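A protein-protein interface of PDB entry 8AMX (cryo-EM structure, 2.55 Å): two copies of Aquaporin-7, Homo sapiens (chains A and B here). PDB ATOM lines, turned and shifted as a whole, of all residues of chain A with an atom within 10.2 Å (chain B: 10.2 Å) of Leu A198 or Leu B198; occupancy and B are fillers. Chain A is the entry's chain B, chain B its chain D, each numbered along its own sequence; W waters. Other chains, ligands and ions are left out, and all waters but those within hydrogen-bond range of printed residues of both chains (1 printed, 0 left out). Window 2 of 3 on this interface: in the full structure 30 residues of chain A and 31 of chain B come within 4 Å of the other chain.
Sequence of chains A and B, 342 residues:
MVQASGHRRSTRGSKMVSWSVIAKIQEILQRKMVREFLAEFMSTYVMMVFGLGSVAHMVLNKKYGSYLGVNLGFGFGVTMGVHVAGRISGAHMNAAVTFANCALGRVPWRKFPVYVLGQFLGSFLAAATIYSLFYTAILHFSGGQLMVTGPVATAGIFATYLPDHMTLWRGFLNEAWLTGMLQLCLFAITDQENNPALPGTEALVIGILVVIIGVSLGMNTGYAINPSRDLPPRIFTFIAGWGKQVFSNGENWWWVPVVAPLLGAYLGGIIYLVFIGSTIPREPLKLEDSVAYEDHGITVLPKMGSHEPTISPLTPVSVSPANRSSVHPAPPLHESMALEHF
His A83 touches Pro B196, but with the chains exchanged Pro A196 does not touch His B83 (21.2 Å).
His A83 touches Val B205, but with the chains exchanged Val A205 does not touch His B83 (17.1 Å).
Leu A198 touches its own counterpart, Leu B198.
Gly A200 touches Ala B197, but with the chains exchanged Ala A197 does not touch Gly B200 (14.3 Å).
18 positions are printed for both chains.
Of the 8 pairs that touch across the chains among the printed residues, 1 has its exchanged pair printed and touching as well.
O of Gly A200 lies within hydrogen-bond range of N of Leu B198 (3.3 Å).
A ring nitrogen (ND1) of His A83 is in hydrogen-bond range of the backbone carbonyl oxygen (O) of Asn B195, at 3.2 Å.
CE1 of His A83 touches C of Pro B196, 3.9 Å away.
CE1 of His A83 touches N of Ala B197, 3.6 Å away.
CG1 of Val B205 touches NE2 of His A83, 3.8 Å away.
CD2 of Leu A198 touches CD2 of Leu B198, 3.8 Å away.
Pro A199 touches Leu B198 (O to CD1, 3.9 Å).
Gly A200 touches Ala B197.
N of Gly A200 is in hydrogen-bond range of OE1 of Glu A202 (3.3 Å).
The backbone carbonyl oxygen (O) of Leu A198 lies within hydrogen-bond range of the side-chain hydroxyl (OG1) of Thr A201 (2.7 Å).
OG1 of Thr B201 sits at hydrogen-bond distance from O of Leu B198.
The backbone NH (N) of Ala B197 is in hydrogen-bond range of the backbone carbonyl oxygen (O) of Ile B189 (3.2 Å).
Water W1 lies within hydrogen-bond range of the backbone carbonyl oxygen (O) of Ala B188 (2.6 Å), the backbone NH (N) of Asn B195 (3.1 Å) and the backbone carbonyl oxygen (O) of His A83 (3.4 Å).
Of the 18 printed residues of chain B, 5 touch a printed residue of chain A.
Hydrophobic or aromatic side chains of chain B within 4 Å of the printed part of chain A: Ala B197, Leu B198 and Val B205.
Leu A198 touches just one residue of chain B: Leu B198.
Ala A197 touches none of the printed residues of chain B.
Pro A199 touches just one residue of chain B: Leu B198.
No residue of chain B comes within 4 Å of Thr A201.
Ala B197 touches just these residues of chain A: His A83 (3.6 Å) and Gly A200 (3.9 Å).
No residue of chain A comes within 4 Å of Pro B199.
No residue of chain A comes within 4 Å of Gly B200.
Of the printed residues of chain A, Pro B196 touches His A83 (3.9 Å).
Of the printed residues of chain A, Val B205 touches His A83.
Of the printed residues of chain B, His A83 touches Asn B195 (3.2 Å), Pro B196 (3.9 Å), Ala B197 (3.6 Å) and Val B205 (3.8 Å).
Printed residues of chain A within 4 Å of Asn B195: His A83.
Ala B203 touches none of the printed residues of chain A.
Leu B204 touches none of the printed residues of chain A.
The nearest residue of chain B that does not touch Leu A198 is Thr B201 (6.9 Å).
The nearest residue of chain A that does not touch Leu B198 is Thr A201 (4.2 Å).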
ATOM      1  N   HIS A  83     -13.348  -0.081  20.991  1.00  0.00           N
ATOM      2  CA  HIS A  83     -14.421  -0.953  20.514  1.00  0.00           C
ATOM      3  C   HIS A  83     -14.972  -0.484  19.173  1.00  0.00           C
ATOM      4  O   HIS A  83     -15.377  -1.301  18.340  1.00  0.00           O
ATOM      5  CB  HIS A  83     -15.542  -1.051  21.546  1.00  0.00           C
ATOM      6  CG  HIS A  83     -15.377  -2.194  22.491  1.00  0.00           C
ATOM      7  ND1 HIS A  83     -15.350  -3.504  22.070  1.00  0.00           N
ATOM      8  CD2 HIS A  83     -15.205  -2.227  23.831  1.00  0.00           C
ATOM      9  CE1 HIS A  83     -15.175  -4.295  23.110  1.00  0.00           C
ATOM     10  NE2 HIS A  83     -15.085  -3.545  24.192  1.00  0.00           N
ATOM     11  N   ALA A 188       3.208  -3.619  25.306  1.00  0.00           N
ATOM     12  CA  ALA A 188       3.129  -4.808  26.153  1.00  0.00           C
ATOM     13  C   ALA A 188       1.739  -5.443  26.124  1.00  0.00           C
ATOM     14  O   ALA A 188       1.616  -6.672  26.107  1.00  0.00           O
ATOM     15  CB  ALA A 188       3.526  -4.463  27.585  1.00  0.00           C
ATOM     16  N   ILE A 189       0.683  -4.626  26.136  1.00  0.00           N
ATOM     17  CA  ILE A 189      -0.673  -5.158  26.263  1.00  0.00           C
ATOM     18  C   ILE A 189      -1.086  -5.927  25.009  1.00  0.00           C
ATOM     19  O   ILE A 189      -1.768  -6.954  25.093  1.00  0.00           O
ATOM     20  CB  ILE A 189      -1.663  -4.023  26.586  1.00  0.00           C
ATOM     21  CG1 ILE A 189      -1.407  -3.461  27.984  1.00  0.00           C
ATOM     22  CG2 ILE A 189      -3.095  -4.508  26.494  1.00  0.00           C
ATOM     23  CD1 ILE A 189      -2.263  -2.263  28.329  1.00  0.00           C
ATOM     24  N   THR A 190      -0.688  -5.452  23.829  1.00  0.00           N
ATOM     25  CA  THR A 190      -1.175  -6.005  22.570  1.00  0.00           C
ATOM     26  C   THR A 190      -0.129  -6.847  21.842  1.00  0.00           C
ATOM     27  O   THR A 190      -0.163  -6.940  20.613  1.00  0.00           O
ATOM     28  CB  THR A 190      -1.668  -4.883  21.655  1.00  0.00           C
ATOM     29  OG1 THR A 190      -0.578  -4.024  21.311  1.00  0.00           O
ATOM     30  CG2 THR A 190      -2.744  -4.063  22.341  1.00  0.00           C
ATOM     31  N   ASP A 191       0.788  -7.483  22.570  1.00  0.00           N
ATOM     32  CA  ASP A 191       1.854  -8.279  21.967  1.00  0.00           C
ATOM     33  C   ASP A 191       1.459  -9.749  22.030  1.00  0.00           C
ATOM     34  O   ASP A 191       1.484 -10.358  23.103  1.00  0.00           O
ATOM     35  CB  ASP A 191       3.185  -8.043  22.675  1.00  0.00           C
ATOM     36  CG  ASP A 191       4.353  -8.671  21.944  1.00  0.00           C
ATOM     37  OD1 ASP A 191       4.181  -9.074  20.777  1.00  0.00           O
ATOM     38  OD2 ASP A 191       5.446  -8.764  22.533  1.00  0.00           O
ATOM     39  N   GLN A 192       1.110 -10.318  20.875  1.00  0.00           N
ATOM     40  CA  GLN A 192       0.626 -11.692  20.826  1.00  0.00           C
ATOM     41  C   GLN A 192       1.718 -12.707  21.121  1.00  0.00           C
ATOM     42  O   GLN A 192       1.407 -13.867  21.405  1.00  0.00           O
ATOM     43  CB  GLN A 192       0.007 -11.988  19.462  1.00  0.00           C
ATOM     44  CG  GLN A 192      -1.216 -11.152  19.156  1.00  0.00           C
ATOM     45  CD  GLN A 192      -2.262 -11.241  20.246  1.00  0.00           C
ATOM     46  OE1 GLN A 192      -2.647 -12.330  20.666  1.00  0.00           O
ATOM     47  NE2 GLN A 192      -2.721 -10.092  20.718  1.00  0.00           N
ATOM     48  N   ASN A 195       2.858 -11.708  26.202  1.00  0.00           N
ATOM     49  CA  ASN A 195       1.886 -11.949  27.269  1.00  0.00           C
ATOM     50  C   ASN A 195       0.708 -10.999  27.106  1.00  0.00           C
ATOM     51  O   ASN A 195       0.488 -10.111  27.936  1.00  0.00           O
ATOM     52  CB  ASN A 195       2.538 -11.779  28.641  1.00  0.00           C
ATOM     53  CG  ASN A 195       1.740 -12.420  29.750  1.00  0.00           C
ATOM     54  OD1 ASN A 195       1.012 -13.380  29.527  1.00  0.00           O
ATOM     55  ND2 ASN A 195       1.875 -11.896  30.955  1.00  0.00           N
ATOM     56  N   PRO A 196      -0.083 -11.168  26.054  1.00  0.00           N
ATOM     57  CA  PRO A 196      -1.132 -10.193  25.764  1.00  0.00           C
ATOM     58  C   PRO A 196      -2.342 -10.360  26.671  1.00  0.00           C
ATOM     59  O   PRO A 196      -2.487 -11.341  27.403  1.00  0.00           O
ATOM     60  CB  PRO A 196      -1.487 -10.502  24.309  1.00  0.00           C
ATOM     61  CG  PRO A 196      -1.251 -11.949  24.195  1.00  0.00           C
ATOM     62  CD  PRO A 196      -0.094 -12.279  25.089  1.00  0.00           C
ATOM     63  N   ALA A 197      -3.209  -9.355  26.621  1.00  0.00           N
ATOM     64  CA  ALA A 197      -4.545  -9.483  27.173  1.00  0.00           C
ATOM     65  C   ALA A 197      -5.379 -10.383  26.272  1.00  0.00           C
ATOM     66  O   ALA A 197      -5.218 -10.388  25.050  1.00  0.00           O
ATOM     67  CB  ALA A 197      -5.205  -8.113  27.312  1.00  0.00           C
ATOM     68  N   LEU A 198      -6.264 -11.155  26.889  1.00  0.00           N
ATOM     69  CA  LEU A 198      -7.065 -12.113  26.144  1.00  0.00           C
ATOM     70  C   LEU A 198      -7.860 -11.386  25.062  1.00  0.00           C
ATOM     71  O   LEU A 198      -8.496 -10.366  25.352  1.00  0.00           O
ATOM     72  CB  LEU A 198      -8.005 -12.862  27.087  1.00  0.00           C
ATOM     73  CG  LEU A 198      -8.873 -13.977  26.502  1.00  0.00           C
ATOM     74  CD1 LEU A 198      -8.017 -15.105  25.952  1.00  0.00           C
ATOM     75  CD2 LEU A 198      -9.831 -14.504  27.543  1.00  0.00           C
ATOM     76  N   PRO A 199      -7.819 -11.849  23.811  1.00  0.00           N
ATOM     77  CA  PRO A 199      -8.530 -11.142  22.741  1.00  0.00           C
ATOM     78  C   PRO A 199     -10.010 -10.994  23.048  1.00  0.00           C
ATOM     79  O   PRO A 199     -10.667 -11.928  23.507  1.00  0.00           O
ATOM     80  CB  PRO A 199      -8.289 -12.030  21.518  1.00  0.00           C
ATOM     81  CG  PRO A 199      -6.983 -12.667  21.799  1.00  0.00           C
ATOM     82  CD  PRO A 199      -6.958 -12.918  23.277  1.00  0.00           C
ATOM     83  N   GLY A 200     -10.531  -9.801  22.776  1.00  0.00           N
ATOM     84  CA  GLY A 200     -11.857  -9.423  23.196  1.00  0.00           C
ATOM     85  C   GLY A 200     -11.924  -8.709  24.528  1.00  0.00           C
ATOM     86  O   GLY A 200     -13.003  -8.243  24.906  1.00  0.00           O
ATOM     87  N   THR A 201     -10.806  -8.607  25.257  1.00  0.00           N
ATOM     88  CA  THR A 201     -10.784  -7.921  26.541  1.00  0.00           C
ATOM     89  C   THR A 201      -9.721  -6.834  26.646  1.00  0.00           C
ATOM     90  O   THR A 201      -9.571  -6.253  27.723  1.00  0.00           O
ATOM     91  CB  THR A 201     -10.570  -8.921  27.696  1.00  0.00           C
ATOM     92  OG1 THR A 201      -9.208  -9.361  27.711  1.00  0.00           O
ATOM     93  CG2 THR A 201     -11.479 -10.130  27.554  1.00  0.00           C
ATOM     94  N   GLU A 202      -8.983  -6.538  25.574  1.00  0.00           N
ATOM     95  CA  GLU A 202      -7.857  -5.615  25.684  1.00  0.00           C
ATOM     96  C   GLU A 202      -8.287  -4.156  25.790  1.00  0.00           C
ATOM     97  O   GLU A 202      -7.521  -3.337  26.313  1.00  0.00           O
ATOM     98  CB  GLU A 202      -6.904  -5.794  24.499  1.00  0.00           C
ATOM     99  CG  GLU A 202      -7.451  -5.347  23.162  1.00  0.00           C
ATOM    100  CD  GLU A 202      -8.176  -6.453  22.419  1.00  0.00           C
ATOM    101  OE1 GLU A 202      -8.014  -7.630  22.797  1.00  0.00           O
ATOM    102  OE2 GLU A 202      -8.903  -6.145  21.452  1.00  0.00           O
ATOM    103  N   ALA A 203      -9.492  -3.815  25.325  1.00  0.00           N
ATOM    104  CA  ALA A 203      -9.965  -2.437  25.417  1.00  0.00           C
ATOM    105  C   ALA A 203     -10.083  -1.984  26.867  1.00  0.00           C
ATOM    106  O   ALA A 203      -9.745  -0.840  27.197  1.00  0.00           O
ATOM    107  CB  ALA A 203     -11.303  -2.298  24.695  1.00  0.00           C
ATOM    108  N   LEU A 204     -10.557  -2.868  27.747  1.00  0.00           N
ATOM    109  CA  LEU A 204     -10.640  -2.537  29.167  1.00  0.00           C
ATOM    110  C   LEU A 204      -9.266  -2.265  29.760  1.00  0.00           C
ATOM    111  O   LEU A 204      -9.096  -1.328  30.550  1.00  0.00           O
ATOM    112  CB  LEU A 204     -11.321  -3.670  29.931  1.00  0.00           C
ATOM    113  CG  LEU A 204     -12.839  -3.760  29.851  1.00  0.00           C
ATOM    114  CD1 LEU A 204     -13.336  -4.919  30.688  1.00  0.00           C
ATOM    115  CD2 LEU A 204     -13.457  -2.460  30.314  1.00  0.00           C
ATOM    116  N   VAL A 205      -8.273  -3.078  29.400  1.00  0.00           N
ATOM    117  CA  VAL A 205      -6.935  -2.908  29.956  1.00  0.00           C
ATOM    118  C   VAL A 205      -6.299  -1.618  29.449  1.00  0.00           C
ATOM    119  O   VAL A 205      -5.610  -0.915  30.196  1.00  0.00           O
ATOM    120  CB  VAL A 205      -6.073  -4.145  29.644  1.00  0.00           C
ATOM    121  CG1 VAL A 205      -4.810  -4.132  30.470  1.00  0.00           C
ATOM    122  CG2 VAL A 205      -6.861  -5.406  29.916  1.00  0.00           C
ATOM    123  N   ILE A 206      -6.528  -1.277  28.178  1.00  0.00           N
ATOM    124  CA  ILE A 206      -6.015  -0.014  27.645  1.00  0.00           C
ATOM    125  C   ILE A 206      -6.671   1.174  28.347  1.00  0.00           C
ATOM    126  O   ILE A 206      -6.004   2.164  28.693  1.00  0.00           O
ATOM    127  CB  ILE A 206      -6.214   0.034  26.119  1.00  0.00           C
ATOM    128  CG1 ILE A 206      -5.424  -1.087  25.445  1.00  0.00           C
ATOM    129  CG2 ILE A 206      -5.790   1.376  25.564  1.00  0.00           C
ATOM    130  CD1 ILE A 206      -5.705  -1.242  23.972  1.00  0.00           C
ATOM    131  N   HIS B  83     -27.356  -9.520  32.796  1.00  0.00           N
ATOM    132  CA  HIS B  83     -27.182 -10.921  33.181  1.00  0.00           C
ATOM    133  C   HIS B  83     -28.522 -11.616  33.389  1.00  0.00           C
ATOM    134  O   HIS B  83     -28.657 -12.813  33.114  1.00  0.00           O
ATOM    135  CB  HIS B  83     -26.321 -11.038  34.437  1.00  0.00           C
ATOM    136  CG  HIS B  83     -24.867 -11.203  34.142  1.00  0.00           C
ATOM    137  ND1 HIS B  83     -24.372 -12.274  33.434  1.00  0.00           N
ATOM    138  CD2 HIS B  83     -23.802 -10.423  34.437  1.00  0.00           C
ATOM    139  CE1 HIS B  83     -23.065 -12.151  33.310  1.00  0.00           C
ATOM    140  NE2 HIS B  83     -22.694 -11.037  33.910  1.00  0.00           N
ATOM    141  N   ALA B 188     -21.722  -0.727  18.789  1.00  0.00           N
ATOM    142  CA  ALA B 188     -20.318  -1.106  18.650  1.00  0.00           C
ATOM    143  C   ALA B 188     -19.946  -2.282  19.551  1.00  0.00           C
ATOM    144  O   ALA B 188     -19.189  -3.167  19.140  1.00  0.00           O
ATOM    145  CB  ALA B 188     -19.419   0.093  18.940  1.00  0.00           C
ATOM    146  N   ILE B 189     -20.453  -2.302  20.787  1.00  0.00           N
ATOM    147  CA  ILE B 189     -20.023  -3.308  21.758  1.00  0.00           C
ATOM    148  C   ILE B 189     -20.514  -4.702  21.365  1.00  0.00           C
ATOM    149  O   ILE B 189     -19.804  -5.696  21.550  1.00  0.00           O
ATOM    150  CB  ILE B 189     -20.489  -2.917  23.172  1.00  0.00           C
ATOM    151  CG1 ILE B 189     -19.753  -1.670  23.660  1.00  0.00           C
ATOM    152  CG2 ILE B 189     -20.263  -4.048  24.152  1.00  0.00           C
ATOM    153  CD1 ILE B 189     -20.238  -1.154  24.997  1.00  0.00           C
ATOM    154  N   THR B 190     -21.728  -4.804  20.827  1.00  0.00           N
ATOM    155  CA  THR B 190     -22.365  -6.094  20.587  1.00  0.00           C
ATOM    156  C   THR B 190     -22.398  -6.481  19.110  1.00  0.00           C
ATOM    157  O   THR B 190     -23.307  -7.198  18.685  1.00  0.00           O
ATOM    158  CB  THR B 190     -23.786  -6.096  21.154  1.00  0.00           C
ATOM    159  OG1 THR B 190     -24.581  -5.127  20.463  1.00  0.00           O
ATOM    160  CG2 THR B 190     -23.781  -5.767  22.632  1.00  0.00           C
ATOM    161  N   ASP B 191     -21.423  -6.042  18.318  1.00  0.00           N
ATOM    162  CA  ASP B 191     -21.400  -6.311  16.883  1.00  0.00           C
ATOM    163  C   ASP B 191     -20.422  -7.444  16.607  1.00  0.00           C
ATOM    164  O   ASP B 191     -19.206  -7.246  16.652  1.00  0.00           O
ATOM    165  CB  ASP B 191     -21.015  -5.061  16.096  1.00  0.00           C
ATOM    166  CG  ASP B 191     -21.172  -5.244  14.601  1.00  0.00           C
ATOM    167  OD1 ASP B 191     -21.823  -6.221  14.185  1.00  0.00           O
ATOM    168  OD2 ASP B 191     -20.643  -4.414  13.838  1.00  0.00           O
ATOM    169  N   GLN B 192     -20.954  -8.628  16.296  1.00  0.00           N
ATOM    170  CA  GLN B 192     -20.106  -9.798  16.110  1.00  0.00           C
ATOM    171  C   GLN B 192     -19.237  -9.699  14.865  1.00  0.00           C
ATOM    172  O   GLN B 192     -18.238 -10.415  14.765  1.00  0.00           O
ATOM    173  CB  GLN B 192     -20.958 -11.064  16.055  1.00  0.00           C
ATOM    174  CG  GLN B 192     -21.751 -11.322  17.322  1.00  0.00           C
ATOM    175  CD  GLN B 192     -20.877 -11.365  18.559  1.00  0.00           C
ATOM    176  OE1 GLN B 192     -19.869 -12.067  18.596  1.00  0.00           O
ATOM    177  NE2 GLN B 192     -21.258 -10.608  19.577  1.00  0.00           N
ATOM    178  N   ASN B 195     -15.992  -5.775  16.006  1.00  0.00           N
ATOM    179  CA  ASN B 195     -15.023  -5.890  17.092  1.00  0.00           C
ATOM    180  C   ASN B 195     -15.741  -5.961  18.432  1.00  0.00           C
ATOM    181  O   ASN B 195     -15.646  -5.026  19.235  1.00  0.00           O
ATOM    182  CB  ASN B 195     -14.047  -4.711  17.079  1.00  0.00           C
ATOM    183  CG  ASN B 195     -12.792  -4.982  17.880  1.00  0.00           C
ATOM    184  OD1 ASN B 195     -12.393  -6.127  18.052  1.00  0.00           O
ATOM    185  ND2 ASN B 195     -12.160  -3.930  18.371  1.00  0.00           N
ATOM    186  N   PRO B 196     -16.449  -7.044  18.719  1.00  0.00           N
ATOM    187  CA  PRO B 196     -17.274  -7.087  19.925  1.00  0.00           C
ATOM    188  C   PRO B 196     -16.460  -7.401  21.172  1.00  0.00           C
ATOM    189  O   PRO B 196     -15.297  -7.802  21.115  1.00  0.00           O
ATOM    190  CB  PRO B 196     -18.263  -8.210  19.617  1.00  0.00           C
ATOM    191  CG  PRO B 196     -17.487  -9.131  18.763  1.00  0.00           C
ATOM    192  CD  PRO B 196     -16.531  -8.302  17.960  1.00  0.00           C
ATOM    193  N   ALA B 197     -17.100  -7.190  22.316  1.00  0.00           N
ATOM    194  CA  ALA B 197     -16.583  -7.725  23.563  1.00  0.00           C
ATOM    195  C   ALA B 197     -16.717  -9.243  23.561  1.00  0.00           C
ATOM    196  O   ALA B 197     -17.638  -9.803  22.963  1.00  0.00           O
ATOM    197  CB  ALA B 197     -17.327  -7.124  24.753  1.00  0.00           C
ATOM    198  N   LEU B 198     -15.783  -9.908  24.228  1.00  0.00           N
ATOM    199  CA  LEU B 198     -15.775 -11.363  24.248  1.00  0.00           C
ATOM    200  C   LEU B 198     -17.080 -11.875  24.848  1.00  0.00           C
ATOM    201  O   LEU B 198     -17.500 -11.387  25.904  1.00  0.00           O
ATOM    202  CB  LEU B 198     -14.579 -11.876  25.050  1.00  0.00           C
ATOM    203  CG  LEU B 198     -14.331 -13.385  25.117  1.00  0.00           C
ATOM    204  CD1 LEU B 198     -14.044 -13.953  23.740  1.00  0.00           C
ATOM    205  CD2 LEU B 198     -13.193 -13.692  26.061  1.00  0.00           C
ATOM    206  N   PRO B 199     -17.761 -12.822  24.199  1.00  0.00           N
ATOM    207  CA  PRO B 199     -19.041 -13.304  24.731  1.00  0.00           C
ATOM    208  C   PRO B 199     -18.900 -13.840  26.147  1.00  0.00           C
ATOM    209  O   PRO B 199     -17.958 -14.565  26.468  1.00  0.00           O
ATOM    210  CB  PRO B 199     -19.434 -14.404  23.744  1.00  0.00           C
ATOM    211  CG  PRO B 199     -18.810 -13.976  22.472  1.00  0.00           C
ATOM    212  CD  PRO B 199     -17.501 -13.347  22.849  1.00  0.00           C
ATOM    213  N   GLY B 200     -19.862 -13.479  26.991  1.00  0.00           N
ATOM    214  CA  GLY B 200     -19.775 -13.716  28.410  1.00  0.00           C
ATOM    215  C   GLY B 200     -19.185 -12.577  29.212  1.00  0.00           C
ATOM    216  O   GLY B 200     -19.185 -12.649  30.445  1.00  0.00           O
ATOM    217  N   THR B 201     -18.682 -11.526  28.557  1.00  0.00           N
ATOM    218  CA  THR B 201     -18.109 -10.383  29.254  1.00  0.00           C
ATOM    219  C   THR B 201     -18.706  -9.043  28.841  1.00  0.00           C
ATOM    220  O   THR B 201     -18.231  -8.011  29.321  1.00  0.00           O
ATOM    221  CB  THR B 201     -16.584 -10.320  29.048  1.00  0.00           C
ATOM    222  OG1 THR B 201     -16.290  -9.874  27.721  1.00  0.00           O
ATOM    223  CG2 THR B 201     -15.938 -11.678  29.268  1.00  0.00           C
ATOM    224  N   GLU B 202     -19.723  -9.021  27.978  1.00  0.00           N
ATOM    225  CA  GLU B 202     -20.213  -7.753  27.444  1.00  0.00           C
ATOM    226  C   GLU B 202     -21.048  -6.964  28.449  1.00  0.00           C
ATOM    227  O   GLU B 202     -21.152  -5.739  28.316  1.00  0.00           O
ATOM    228  CB  GLU B 202     -21.019  -7.990  26.165  1.00  0.00           C
ATOM    229  CG  GLU B 202     -22.342  -8.694  26.362  1.00  0.00           C
ATOM    230  CD  GLU B 202     -22.230 -10.202  26.267  1.00  0.00           C
ATOM    231  OE1 GLU B 202     -21.196 -10.691  25.770  1.00  0.00           O
ATOM    232  OE2 GLU B 202     -23.178 -10.900  26.682  1.00  0.00           O
ATOM    233  N   ALA B 203     -21.627  -7.628  29.451  1.00  0.00           N
ATOM    234  CA  ALA B 203     -22.422  -6.925  30.453  1.00  0.00           C
ATOM    235  C   ALA B 203     -21.578  -5.921  31.230  1.00  0.00           C
ATOM    236  O   ALA B 203     -22.037  -4.811  31.529  1.00  0.00           O
ATOM    237  CB  ALA B 203     -23.076  -7.929  31.399  1.00  0.00           C
ATOM    238  N   LEU B 204     -20.339  -6.290  31.561  1.00  0.00           N
ATOM    239  CA  LEU B 204     -19.442  -5.366  32.247  1.00  0.00           C
ATOM    240  C   LEU B 204     -19.146  -4.138  31.398  1.00  0.00           C
ATOM    241  O   LEU B 204     -19.120  -3.012  31.908  1.00  0.00           O
ATOM    242  CB  LEU B 204     -18.138  -6.072  32.611  1.00  0.00           C
ATOM    243  CG  LEU B 204     -18.148  -6.984  33.831  1.00  0.00           C
ATOM    244  CD1 LEU B 204     -16.771  -7.569  34.055  1.00  0.00           C
ATOM    245  CD2 LEU B 204     -18.605  -6.211  35.047  1.00  0.00           C
ATOM    246  N   VAL B 205     -18.912  -4.334  30.100  1.00  0.00           N
ATOM    247  CA  VAL B 205     -18.581  -3.213  29.228  1.00  0.00           C
ATOM    248  C   VAL B 205     -19.785  -2.292  29.053  1.00  0.00           C
ATOM    249  O   VAL B 205     -19.641  -1.065  29.013  1.00  0.00           O
ATOM    250  CB  VAL B 205     -18.046  -3.734  27.882  1.00  0.00           C
ATOM    251  CG1 VAL B 205     -17.407  -2.614  27.098  1.00  0.00           C
ATOM    252  CG2 VAL B 205     -17.045  -4.842  28.118  1.00  0.00           C
ATOM    253  N   ILE B 206     -20.989  -2.862  28.959  1.00  0.00           N
ATOM    254  CA  ILE B 206     -22.194  -2.038  28.868  1.00  0.00           C
ATOM    255  C   ILE B 206     -22.396  -1.234  30.151  1.00  0.00           C
ATOM    256  O   ILE B 206     -22.746  -0.041  30.114  1.00  0.00           O
ATOM    257  CB  ILE B 206     -23.414  -2.920  28.542  1.00  0.00           C
ATOM    258  CG1 ILE B 206     -23.233  -3.595  27.182  1.00  0.00           C
ATOM    259  CG2 ILE B 206     -24.687  -2.104  28.552  1.00  0.00           C
ATOM    260  CD1 ILE B 206     -24.282  -4.625  26.859  1.00  0.00           C
HETATM  261  O   HOH W   1     -17.681  -3.430  17.081  1.00  0.00           O
